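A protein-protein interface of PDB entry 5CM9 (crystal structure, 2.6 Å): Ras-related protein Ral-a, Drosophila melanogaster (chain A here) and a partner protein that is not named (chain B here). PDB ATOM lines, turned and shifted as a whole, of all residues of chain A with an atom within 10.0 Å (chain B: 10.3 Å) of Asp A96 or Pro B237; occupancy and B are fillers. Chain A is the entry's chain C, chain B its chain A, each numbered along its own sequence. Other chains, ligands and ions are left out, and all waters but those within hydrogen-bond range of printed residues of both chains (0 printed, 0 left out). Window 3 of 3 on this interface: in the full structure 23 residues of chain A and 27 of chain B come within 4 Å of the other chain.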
ATOM      1  N   SER A  21       1.335  -1.328  27.425  1.00  0.00           N
ATOM      2  CA  SER A  21       2.773  -1.274  27.200  1.00  0.00           C
ATOM      3  C   SER A  21       3.075  -1.368  25.707  1.00  0.00           C
ATOM      4  O   SER A  21       2.196  -1.696  24.907  1.00  0.00           O
ATOM      5  CB  SER A  21       3.461  -2.415  27.953  1.00  0.00           C
ATOM      6  OG  SER A  21       4.849  -2.439  27.682  1.00  0.00           O
ATOM      7  N   GLY A  22       4.317  -1.067  25.334  1.00  0.00           N
ATOM      8  CA  GLY A  22       4.778  -1.260  23.961  1.00  0.00           C
ATOM      9  C   GLY A  22       4.910  -2.740  23.641  1.00  0.00           C
ATOM     10  O   GLY A  22       5.235  -3.547  24.519  1.00  0.00           O
ATOM     11  N   GLY A  23       4.649  -3.095  22.385  1.00  0.00           N
ATOM     12  CA  GLY A  23       4.736  -4.485  21.929  1.00  0.00           C
ATOM     13  C   GLY A  23       3.493  -5.308  22.216  1.00  0.00           C
ATOM     14  O   GLY A  23       3.397  -6.467  21.803  1.00  0.00           O
ATOM     15  N   VAL A  24       2.546  -4.707  22.931  1.00  0.00           N
ATOM     16  CA  VAL A  24       1.274  -5.340  23.262  1.00  0.00           C
ATOM     17  C   VAL A  24       0.368  -5.370  22.027  1.00  0.00           C
ATOM     18  O   VAL A  24      -0.381  -6.327  21.814  1.00  0.00           O
ATOM     19  CB  VAL A  24       0.581  -4.606  24.433  1.00  0.00           C
ATOM     20  CG1 VAL A  24      -0.836  -5.101  24.625  1.00  0.00           C
ATOM     21  CG2 VAL A  24       1.382  -4.771  25.721  1.00  0.00           C
ATOM     22  N   GLY A  25       0.449  -4.318  21.217  1.00  0.00           N
ATOM     23  CA  GLY A  25      -0.312  -4.242  19.979  1.00  0.00           C
ATOM     24  C   GLY A  25      -1.653  -3.557  20.138  1.00  0.00           C
ATOM     25  O   GLY A  25      -2.655  -4.024  19.598  1.00  0.00           O
ATOM     26  N   VAL A  91      -4.992  -2.599  27.704  1.00  0.00           N
ATOM     27  CA  VAL A  91      -4.515  -3.690  26.851  1.00  0.00           C
ATOM     28  C   VAL A  91      -3.167  -4.264  27.311  1.00  0.00           C
ATOM     29  O   VAL A  91      -2.199  -3.525  27.523  1.00  0.00           O
ATOM     30  CB  VAL A  91      -4.446  -3.271  25.350  1.00  0.00           C
ATOM     31  CG1 VAL A  91      -4.429  -4.495  24.454  1.00  0.00           C
ATOM     32  CG2 VAL A  91      -5.626  -2.382  24.976  1.00  0.00           C
ATOM     33  N   PHE A  92      -3.131  -5.587  27.463  1.00  0.00           N
ATOM     34  CA  PHE A  92      -1.913  -6.333  27.787  1.00  0.00           C
ATOM     35  C   PHE A  92      -1.854  -7.591  26.918  1.00  0.00           C
ATOM     36  O   PHE A  92      -2.891  -8.086  26.471  1.00  0.00           O
ATOM     37  CB  PHE A  92      -1.882  -6.706  29.277  1.00  0.00           C
ATOM     38  CG  PHE A  92      -2.874  -7.776  29.661  1.00  0.00           C
ATOM     39  CD1 PHE A  92      -2.491  -9.115  29.707  1.00  0.00           C
ATOM     40  CD2 PHE A  92      -4.193  -7.447  29.969  1.00  0.00           C
ATOM     41  CE1 PHE A  92      -3.407 -10.108  30.052  1.00  0.00           C
ATOM     42  CE2 PHE A  92      -5.115  -8.433  30.316  1.00  0.00           C
ATOM     43  CZ  PHE A  92      -4.721  -9.764  30.361  1.00  0.00           C
ATOM     44  N   SER A  93      -0.651  -8.109  26.683  1.00  0.00           N
ATOM     45  CA  SER A  93      -0.487  -9.334  25.895  1.00  0.00           C
ATOM     46  C   SER A  93      -0.588 -10.589  26.764  1.00  0.00           C
ATOM     47  O   SER A  93      -0.156 -10.592  27.919  1.00  0.00           O
ATOM     48  CB  SER A  93       0.833  -9.320  25.116  1.00  0.00           C
ATOM     49  OG  SER A  93       1.943  -9.552  25.970  1.00  0.00           O
ATOM     50  N   ILE A  94      -1.156 -11.652  26.196  1.00  0.00           N
ATOM     51  CA  ILE A  94      -1.328 -12.925  26.908  1.00  0.00           C
ATOM     52  C   ILE A  94      -0.030 -13.756  26.922  1.00  0.00           C
ATOM     53  O   ILE A  94       0.003 -14.865  27.462  1.00  0.00           O
ATOM     54  CB  ILE A  94      -2.532 -13.745  26.345  1.00  0.00           C
ATOM     55  CG1 ILE A  94      -3.740 -12.828  26.122  1.00  0.00           C
ATOM     56  CG2 ILE A  94      -2.908 -14.891  27.294  1.00  0.00           C
ATOM     57  CD1 ILE A  94      -4.862 -13.444  25.309  1.00  0.00           C
ATOM     58  N   THR A  95       1.033 -13.198  26.342  1.00  0.00           N
ATOM     59  CA  THR A  95       2.347 -13.847  26.302  1.00  0.00           C
ATOM     60  C   THR A  95       3.240 -13.392  27.463  1.00  0.00           C
ATOM     61  O   THR A  95       3.801 -14.222  28.186  1.00  0.00           O
ATOM     62  CB  THR A  95       3.074 -13.584  24.956  1.00  0.00           C
ATOM     63  OG1 THR A  95       2.184 -13.853  23.866  1.00  0.00           O
ATOM     64  CG2 THR A  95       4.314 -14.466  24.820  1.00  0.00           C
ATOM     65  N   ASP A  96       3.360 -12.079  27.639  1.00  0.00           N
ATOM     66  CA  ASP A  96       4.275 -11.516  28.628  1.00  0.00           C
ATOM     67  C   ASP A  96       3.630 -11.327  29.996  1.00  0.00           C
ATOM     68  O   ASP A  96       2.485 -10.879  30.104  1.00  0.00           O
ATOM     69  CB  ASP A  96       4.857 -10.189  28.131  1.00  0.00           C
ATOM     70  CG  ASP A  96       5.732 -10.361  26.901  1.00  0.00           C
ATOM     71  OD1 ASP A  96       6.881 -10.836  27.039  1.00  0.00           O
ATOM     72  OD2 ASP A  96       5.266 -10.015  25.793  1.00  0.00           O
ATOM     73  N   ASP A  97       4.381 -11.684  31.034  1.00  0.00           N
ATOM     74  CA  ASP A  97       3.969 -11.448  32.412  1.00  0.00           C
ATOM     75  C   ASP A  97       4.159  -9.971  32.745  1.00  0.00           C
ATOM     76  O   ASP A  97       3.359  -9.384  33.479  1.00  0.00           O
ATOM     77  CB  ASP A  97       4.787 -12.313  33.382  1.00  0.00           C
ATOM     78  CG  ASP A  97       4.766 -13.793  33.018  1.00  0.00           C
ATOM     79  OD1 ASP A  97       5.474 -14.188  32.064  1.00  0.00           O
ATOM     80  OD2 ASP A  97       4.054 -14.563  33.701  1.00  0.00           O
ATOM     81  N   GLU A  98       5.219  -9.384  32.183  1.00  0.00           N
ATOM     82  CA  GLU A  98       5.613  -7.995  32.443  1.00  0.00           C
ATOM     83  C   GLU A  98       4.563  -6.982  31.983  1.00  0.00           C
ATOM     84  O   GLU A  98       4.245  -6.040  32.714  1.00  0.00           O
ATOM     85  CB  GLU A  98       6.971  -7.689  31.793  1.00  0.00           C
ATOM     86  CG  GLU A  98       8.157  -8.434  32.423  1.00  0.00           C
ATOM     87  CD  GLU A  98       9.439  -8.362  31.575  1.00  0.00           C
ATOM     88  OE1 GLU A  98       9.512  -7.545  30.620  1.00  0.00           O
ATOM     89  OE2 GLU A  98      10.386  -9.130  31.873  1.00  0.00           O
ATOM     90  N   SER A  99       4.029  -7.192  30.779  1.00  0.00           N
ATOM     91  CA  SER A  99       2.996  -6.324  30.201  1.00  0.00           C
ATOM     92  C   SER A  99       1.669  -6.426  30.947  1.00  0.00           C
ATOM     93  O   SER A  99       0.912  -5.459  31.007  1.00  0.00           O
ATOM     94  CB  SER A  99       2.782  -6.662  28.725  1.00  0.00           C
ATOM     95  OG  SER A  99       2.288  -7.982  28.573  1.00  0.00           O
ATOM     96  N   PHE A 100       1.397  -7.608  31.498  1.00  0.00           N
ATOM     97  CA  PHE A 100       0.220  -7.842  32.328  1.00  0.00           C
ATOM     98  C   PHE A 100       0.398  -7.212  33.710  1.00  0.00           C
ATOM     99  O   PHE A 100      -0.563  -6.716  34.298  1.00  0.00           O
ATOM    100  CB  PHE A 100      -0.060  -9.345  32.439  1.00  0.00           C
ATOM    101  CG  PHE A 100      -1.095  -9.708  33.474  1.00  0.00           C
ATOM    102  CD1 PHE A 100      -2.434  -9.372  33.295  1.00  0.00           C
ATOM    103  CD2 PHE A 100      -0.729 -10.407  34.622  1.00  0.00           C
ATOM    104  CE1 PHE A 100      -3.392  -9.717  34.250  1.00  0.00           C
ATOM    105  CE2 PHE A 100      -1.679 -10.756  35.580  1.00  0.00           C
ATOM    106  CZ  PHE A 100      -3.011 -10.412  35.392  1.00  0.00           C
ATOM    107  N   GLN A 101       1.632  -7.226  34.212  1.00  0.00           N
ATOM    108  CA  GLN A 101       1.969  -6.637  35.514  1.00  0.00           C
ATOM    109  C   GLN A 101       1.795  -5.113  35.545  1.00  0.00           C
ATOM    110  O   GLN A 101       1.450  -4.544  36.583  1.00  0.00           O
ATOM    111  CB  GLN A 101       3.394  -7.022  35.921  1.00  0.00           C
ATOM    112  N   ALA A 102       2.029  -4.471  34.402  1.00  0.00           N
ATOM    113  CA  ALA A 102       1.929  -3.013  34.274  1.00  0.00           C
ATOM    114  C   ALA A 102       0.487  -2.487  34.206  1.00  0.00           C
ATOM    115  O   ALA A 102       0.269  -1.275  34.265  1.00  0.00           O
ATOM    116  CB  ALA A 102       2.733  -2.530  33.061  1.00  0.00           C
ATOM    117  N   THR A 103      -0.482  -3.398  34.102  1.00  0.00           N
ATOM    118  CA  THR A 103      -1.892  -3.039  33.921  1.00  0.00           C
ATOM    119  C   THR A 103      -2.503  -2.337  35.137  1.00  0.00           C
ATOM    120  O   THR A 103      -3.405  -1.509  34.994  1.00  0.00           O
ATOM    121  CB  THR A 103      -2.749  -4.273  33.515  1.00  0.00           C
ATOM    122  OG1 THR A 103      -3.793  -3.866  32.624  1.00  0.00           O
ATOM    123  CG2 THR A 103      -3.366  -4.957  34.725  1.00  0.00           C
ATOM    124  N   VAL A 124      -8.160  -5.901  28.451  1.00  0.00           N
ATOM    125  CA  VAL A 124      -8.001  -6.567  27.158  1.00  0.00           C
ATOM    126  C   VAL A 124      -6.716  -7.394  27.074  1.00  0.00           C
ATOM    127  O   VAL A 124      -5.608  -6.853  27.114  1.00  0.00           O
ATOM    128  CB  VAL A 124      -8.068  -5.558  25.973  1.00  0.00           C
ATOM    129  CG1 VAL A 124      -7.842  -6.265  24.640  1.00  0.00           C
ATOM    130  CG2 VAL A 124      -9.403  -4.827  25.955  1.00  0.00           C
ATOM    131  N   GLY A 125      -6.886  -8.707  26.962  1.00  0.00           N
ATOM    132  CA  GLY A 125      -5.781  -9.618  26.687  1.00  0.00           C
ATOM    133  C   GLY A 125      -5.606  -9.757  25.188  1.00  0.00           C
ATOM    134  O   GLY A 125      -6.584  -9.918  24.454  1.00  0.00           O
ATOM    135  N   ASN A 126      -4.359  -9.692  24.731  1.00  0.00           N
ATOM    136  CA  ASN A 126      -4.061  -9.737  23.302  1.00  0.00           C
ATOM    137  C   ASN A 126      -3.060 -10.838  22.940  1.00  0.00           C
ATOM    138  O   ASN A 126      -1.881 -10.767  23.292  1.00  0.00           O
ATOM    139  CB  ASN A 126      -3.578  -8.363  22.815  1.00  0.00           C
ATOM    140  CG  ASN A 126      -3.783  -8.161  21.318  1.00  0.00           C
ATOM    141  OD1 ASN A 126      -2.851  -7.796  20.600  1.00  0.00           O
ATOM    142  ND2 ASN A 126      -5.004  -8.391  20.845  1.00  0.00           N
ATOM    143  N   LYS A 127      -3.549 -11.856  22.238  1.00  0.00           N
ATOM    144  CA  LYS A 127      -2.722 -12.990  21.829  1.00  0.00           C
ATOM    145  C   LYS A 127      -2.097 -12.760  20.455  1.00  0.00           C
ATOM    146  O   LYS A 127      -2.763 -12.285  19.530  1.00  0.00           O
ATOM    147  CB  LYS A 127      -3.543 -14.278  21.836  1.00  0.00           C
ATOM    148  N   CYS A 128      -0.814 -13.097  20.336  1.00  0.00           N
ATOM    149  CA  CYS A 128      -0.092 -12.993  19.071  1.00  0.00           C
ATOM    150  C   CYS A 128       0.961 -14.092  18.943  1.00  0.00           C
ATOM    151  O   CYS A 128       0.638 -15.246  18.658  1.00  0.00           O
ATOM    152  CB  CYS A 128       0.561 -11.616  18.938  1.00  0.00           C
ATOM    153  SG  CYS A 128       1.176 -11.243  17.280  1.00  0.00           S
ATOM    154  N   LYS A 135       1.728 -16.949  27.881  1.00  0.00           N
ATOM    155  CA  LYS A 135       2.176 -17.658  29.075  1.00  0.00           C
ATOM    156  C   LYS A 135       1.290 -17.387  30.295  1.00  0.00           C
ATOM    157  O   LYS A 135       0.966 -18.314  31.041  1.00  0.00           O
ATOM    158  CB  LYS A 135       3.635 -17.327  29.380  1.00  0.00           C
ATOM    159  N   VAL A 136       0.899 -16.124  30.490  1.00  0.00           N
ATOM    160  CA  VAL A 136       0.045 -15.721  31.619  1.00  0.00           C
ATOM    161  C   VAL A 136      -1.354 -16.377  31.556  1.00  0.00           C
ATOM    162  O   VAL A 136      -2.083 -16.202  30.575  1.00  0.00           O
ATOM    163  CB  VAL A 136      -0.017 -14.159  31.787  1.00  0.00           C
ATOM    164  CG1 VAL A 136      -0.471 -13.468  30.505  1.00  0.00           C
ATOM    165  CG2 VAL A 136      -0.896 -13.751  32.965  1.00  0.00           C
ATOM    166  N   PRO A 137      -1.713 -17.150  32.604  1.00  0.00           N
ATOM    167  CA  PRO A 137      -2.936 -17.965  32.656  1.00  0.00           C
ATOM    168  C   PRO A 137      -4.230 -17.165  32.526  1.00  0.00           C
ATOM    169  O   PRO A 137      -4.268 -15.982  32.864  1.00  0.00           O
ATOM    170  CB  PRO A 137      -2.866 -18.619  34.042  1.00  0.00           C
ATOM    171  CG  PRO A 137      -1.430 -18.606  34.395  1.00  0.00           C
ATOM    172  CD  PRO A 137      -0.903 -17.327  33.825  1.00  0.00           C
ATOM    173  N   CYS A 141      -6.163 -13.972  34.674  1.00  0.00           N
ATOM    174  CA  CYS A 141      -6.713 -12.840  33.921  1.00  0.00           C
ATOM    175  C   CYS A 141      -8.114 -12.476  34.411  1.00  0.00           C
ATOM    176  O   CYS A 141      -8.477 -11.299  34.462  1.00  0.00           O
ATOM    177  CB  CYS A 141      -6.762 -13.157  32.422  1.00  0.00           C
ATOM    178  SG  CYS A 141      -5.156 -13.341  31.619  1.00  0.00           S
ATOM    179  N   ARG A 144      -8.307 -10.363  38.081  1.00  0.00           N
ATOM    180  CA  ARG A 144      -8.248  -8.896  38.056  1.00  0.00           C
ATOM    181  C   ARG A 144      -9.529  -8.271  37.508  1.00  0.00           C
ATOM    182  O   ARG A 144      -9.899  -7.162  37.894  1.00  0.00           O
ATOM    183  CB  ARG A 144      -7.026  -8.400  37.277  1.00  0.00           C
ATOM    184  CG  ARG A 144      -5.725  -8.498  38.062  1.00  0.00           C
ATOM    185  CD  ARG A 144      -4.558  -7.851  37.332  1.00  0.00           C
ATOM    186  NE  ARG A 144      -3.301  -8.075  38.050  1.00  0.00           N
ATOM    187  CZ  ARG A 144      -2.089  -7.804  37.566  1.00  0.00           C
ATOM    188  NH1 ARG A 144      -1.944  -7.297  36.343  1.00  0.00           N
ATOM    189  NH2 ARG A 144      -1.014  -8.049  38.306  1.00  0.00           N
ATOM    190  N   GLY B 232       9.027  -0.154  19.627  1.00  0.00           N
ATOM    191  CA  GLY B 232       7.841  -0.901  20.034  1.00  0.00           C
ATOM    192  C   GLY B 232       8.138  -2.105  20.912  1.00  0.00           C
ATOM    193  O   GLY B 232       7.313  -2.484  21.738  1.00  0.00           O
ATOM    194  N   HIS B 233       9.316  -2.701  20.747  1.00  0.00           N
ATOM    195  CA  HIS B 233       9.678  -3.901  21.503  1.00  0.00           C
ATOM    196  C   HIS B 233      10.666  -3.640  22.641  1.00  0.00           C
ATOM    197  O   HIS B 233      11.290  -4.573  23.150  1.00  0.00           O
ATOM    198  CB  HIS B 233      10.227  -4.989  20.568  1.00  0.00           C
ATOM    199  CG  HIS B 233       9.218  -5.525  19.598  1.00  0.00           C
ATOM    200  ND1 HIS B 233       9.497  -5.705  18.259  1.00  0.00           N
ATOM    201  CD2 HIS B 233       7.931  -5.914  19.771  1.00  0.00           C
ATOM    202  CE1 HIS B 233       8.427  -6.186  17.650  1.00  0.00           C
ATOM    203  NE2 HIS B 233       7.462  -6.319  18.544  1.00  0.00           N
ATOM    204  N   ARG B 234      10.794  -2.380  23.051  1.00  0.00           N
ATOM    205  CA  ARG B 234      11.751  -1.995  24.092  1.00  0.00           C
ATOM    206  C   ARG B 234      11.474  -2.669  25.438  1.00  0.00           C
ATOM    207  O   ARG B 234      12.396  -2.885  26.230  1.00  0.00           O
ATOM    208  CB  ARG B 234      11.785  -0.473  24.260  1.00  0.00           C
ATOM    209  CG  ARG B 234      10.556   0.114  24.926  1.00  0.00           C
ATOM    210  CD  ARG B 234      10.521   1.609  24.759  1.00  0.00           C
ATOM    211  NE  ARG B 234       9.302   2.197  25.301  1.00  0.00           N
ATOM    212  CZ  ARG B 234       8.148   2.279  24.649  1.00  0.00           C
ATOM    213  NH1 ARG B 234       8.033   1.805  23.415  1.00  0.00           N
ATOM    214  NH2 ARG B 234       7.101   2.836  25.238  1.00  0.00           N
ATOM    215  N   ASP B 235      10.208  -3.004  25.681  1.00  0.00           N
ATOM    216  CA  ASP B 235       9.785  -3.577  26.956  1.00  0.00           C
ATOM    217  C   ASP B 235       9.969  -5.093  27.026  1.00  0.00           C
ATOM    218  O   ASP B 235      10.095  -5.652  28.117  1.00  0.00           O
ATOM    219  CB  ASP B 235       8.335  -3.184  27.266  1.00  0.00           C
ATOM    220  CG  ASP B 235       8.151  -1.673  27.397  1.00  0.00           C
ATOM    221  OD1 ASP B 235       9.100  -0.979  27.835  1.00  0.00           O
ATOM    222  OD2 ASP B 235       7.053  -1.177  27.061  1.00  0.00           O
ATOM    223  N   ARG B 236       9.993  -5.744  25.862  1.00  0.00           N
ATOM    224  CA  ARG B 236      10.199  -7.197  25.752  1.00  0.00           C
ATOM    225  C   ARG B 236      11.405  -7.714  26.568  1.00  0.00           C
ATOM    226  O   ARG B 236      12.427  -7.032  26.659  1.00  0.00           O
ATOM    227  CB  ARG B 236      10.320  -7.614  24.279  1.00  0.00           C
ATOM    228  CG  ARG B 236       8.991  -7.879  23.575  1.00  0.00           C
ATOM    229  CD  ARG B 236       9.218  -8.778  22.360  1.00  0.00           C
ATOM    230  NE  ARG B 236       7.995  -9.426  21.878  1.00  0.00           N
ATOM    231  CZ  ARG B 236       7.969 -10.524  21.120  1.00  0.00           C
ATOM    232  NH1 ARG B 236       9.100 -11.119  20.755  1.00  0.00           N
ATOM    233  NH2 ARG B 236       6.809 -11.036  20.732  1.00  0.00           N
ATOM    234  N   PRO B 237      11.276  -8.928  27.154  1.00  0.00           N
ATOM    235  CA  PRO B 237      12.153  -9.541  28.172  1.00  0.00           C
ATOM    236  C   PRO B 237      13.676  -9.578  27.945  1.00  0.00           C
ATOM    237  O   PRO B 237      14.391 -10.142  28.779  1.00  0.00           O
ATOM    238  CB  PRO B 237      11.610 -10.969  28.270  1.00  0.00           C
ATOM    239  CG  PRO B 237      10.172 -10.818  27.982  1.00  0.00           C
ATOM    240  CD  PRO B 237      10.109  -9.792  26.882  1.00  0.00           C
ATOM    241  N   GLY B 238      14.173  -8.991  26.859  1.00  0.00           N
ATOM    242  CA  GLY B 238      15.615  -8.937  26.623  1.00  0.00           C
ATOM    243  C   GLY B 238      16.108  -7.660  25.966  1.00  0.00           C
ATOM    244  O   GLY B 238      17.233  -7.612  25.456  1.00  0.00           O
ATOM    245  N   HIS B 239      15.276  -6.620  25.991  1.00  0.00           N
ATOM    246  CA  HIS B 239      15.562  -5.384  25.258  1.00  0.00           C
ATOM    247  C   HIS B 239      15.803  -4.166  26.158  1.00  0.00           C
ATOM    248  O   HIS B 239      15.516  -3.028  25.769  1.00  0.00           O
ATOM    249  CB  HIS B 239      14.440  -5.092  24.253  1.00  0.00           C
ATOM    250  CG  HIS B 239      14.339  -6.096  23.146  1.00  0.00           C
ATOM    251  ND1 HIS B 239      15.339  -6.283  22.215  1.00  0.00           N
ATOM    252  CD2 HIS B 239      13.350  -6.960  22.814  1.00  0.00           C
ATOM    253  CE1 HIS B 239      14.972  -7.223  21.362  1.00  0.00           C
ATOM    254  NE2 HIS B 239      13.769  -7.648  21.701  1.00  0.00           N
ATOM    255  N   SER B 240      16.345  -4.407  27.350  1.00  0.00           N
ATOM    256  CA  SER B 240      16.609  -3.332  28.311  1.00  0.00           C
ATOM    257  C   SER B 240      17.746  -2.396  27.879  1.00  0.00           C
ATOM    258  O   SER B 240      17.775  -1.224  28.279  1.00  0.00           O
ATOM    259  CB  SER B 240      16.892  -3.910  29.702  1.00  0.00           C
ATOM    260  OG  SER B 240      15.745  -4.563  30.224  1.00  0.00           O
ATOM    261  N   HIS B 241      18.668  -2.910  27.064  1.00  0.00           N
ATOM    262  CA  HIS B 241      19.803  -2.121  26.570  1.00  0.00           C
ATOM    263  C   HIS B 241      19.561  -1.632  25.134  1.00  0.00           C
ATOM    264  O   HIS B 241      20.423  -0.982  24.531  1.00  0.00           O
ATOM    265  CB  HIS B 241      21.103  -2.933  26.666  1.00  0.00           C
ATOM    266  CG  HIS B 241      22.335  -2.096  26.851  1.00  0.00           C
ATOM    267  ND1 HIS B 241      22.776  -1.681  28.090  1.00  0.00           N
ATOM    268  CD2 HIS B 241      23.229  -1.613  25.954  1.00  0.00           C
ATOM    269  CE1 HIS B 241      23.881  -0.971  27.950  1.00  0.00           C
ATOM    270  NE2 HIS B 241      24.178  -0.914  26.663  1.00  0.00           N
ATOM    271  N   LEU B 242      18.380  -1.939  24.598  1.00  0.00           N
ATOM    272  CA  LEU B 242      18.011  -1.514  23.252  1.00  0.00           C
ATOM    273  C   LEU B 242      17.443  -0.086  23.236  1.00  0.00           C
ATOM    274  O   LEU B 242      16.733   0.326  24.164  1.00  0.00           O
ATOM    275  CB  LEU B 242      17.006  -2.498  22.641  1.00  0.00           C
ATOM    276  CG  LEU B 242      16.905  -2.576  21.109  1.00  0.00           C
ATOM    277  CD1 LEU B 242      18.059  -3.383  20.500  1.00  0.00           C
ATOM    278  CD2 LEU B 242      15.562  -3.165  20.689  1.00  0.00           C
ATOM    279  N   ARG B 247      15.728   6.530  24.670  1.00  0.00           N
ATOM    280  CA  ARG B 247      15.454   6.494  26.111  1.00  0.00           C
ATOM    281  C   ARG B 247      16.067   7.678  26.849  1.00  0.00           C
ATOM    282  O   ARG B 247      15.438   8.254  27.737  1.00  0.00           O
ATOM    283  CB  ARG B 247      15.956   5.190  26.732  1.00  0.00           C
ATOM    284  CG  ARG B 247      15.228   3.963  26.244  1.00  0.00           C
ATOM    285  CD  ARG B 247      15.508   2.777  27.126  1.00  0.00           C
ATOM    286  NE  ARG B 247      14.559   1.698  26.864  1.00  0.00           N
ATOM    287  CZ  ARG B 247      14.389   0.633  27.641  1.00  0.00           C
ATOM    288  NH1 ARG B 247      15.106   0.485  28.753  1.00  0.00           N
ATOM    289  NH2 ARG B 247      13.496  -0.288  27.303  1.00  0.00           N
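Of the 12 printed residues of chain B, 3 touch a printed residue of chain A. Printed residues of chain B that touch a printed residue of chain A: Gly B232, Asp B235 and Pro B237. Hydrophobic or aromatic side chains of chain B that line the printed part of chain A: Pro B237. Printed residues of chain A that touch a printed residue of chain B: Ser A21, Gly A22, Gly A23, Asp A96 and Glu A98. Among the printed residues, 6 pairs touch across the chains. Among the printed residues, no Asp or Glu carboxylate lies within 4 Å of a Lys or Arg side-chain nitrogen of the other chain.
N of Asp A96 lies within hydrogen-bond range of OG of Ser A93 (3.3 Å). The backbone carbonyl oxygen of Asp A96 sits at hydrogen-bond distance from the side-chain hydroxyl of Ser A99, 3.3 Å away.
Printed residues of chain B within 4 Å of Ser A21: Asp B235 (2.6 Å). Of the printed residues of chain B, Gly A22 touches Gly B232 and Asp B235. Of the printed residues of chain B, Gly A23 touches Gly B232. Asp A96 touches just one residue of chain B: Pro B237 (3.4 Å). No residue of chain B comes within 4 Å of Asp A97. Of chain B, only Asp B235 comes within 4 Å of Glu A98. No residue of chain B comes within 4 Å of Ser A99. Arg A144 touches none of the printed residues of chain B. Of chain A, only Asp A96 comes within 4 Å of Pro B237. No residue of chain A comes within 4 Å of Gly B238. His B239 touches none of the printed residues of chain A. The nearest residue of chain B that does not touch Asp A96 is Arg B236 (4.8 Å).
The side-chain carboxylate of Glu A98 lies close to the backbone carbonyl oxygen of Asp B235. The backbone carbonyl oxygen (O) of Gly B232 lies within hydrogen-bond range of the backbone NH (N) of Gly A23 (2.8 Å). The side-chain carboxylate (OD2) of Asp B235 lies within hydrogen-bond range of the backbone NH (N) of Gly A22 (3.2 Å). OG of Ser A21 is in hydrogen-bond range of OD2 of Asp B235.
Among the printed residues, pairs that only touch across the chains: Gly A22 with Gly B232 and Asp A96 with Pro B237.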
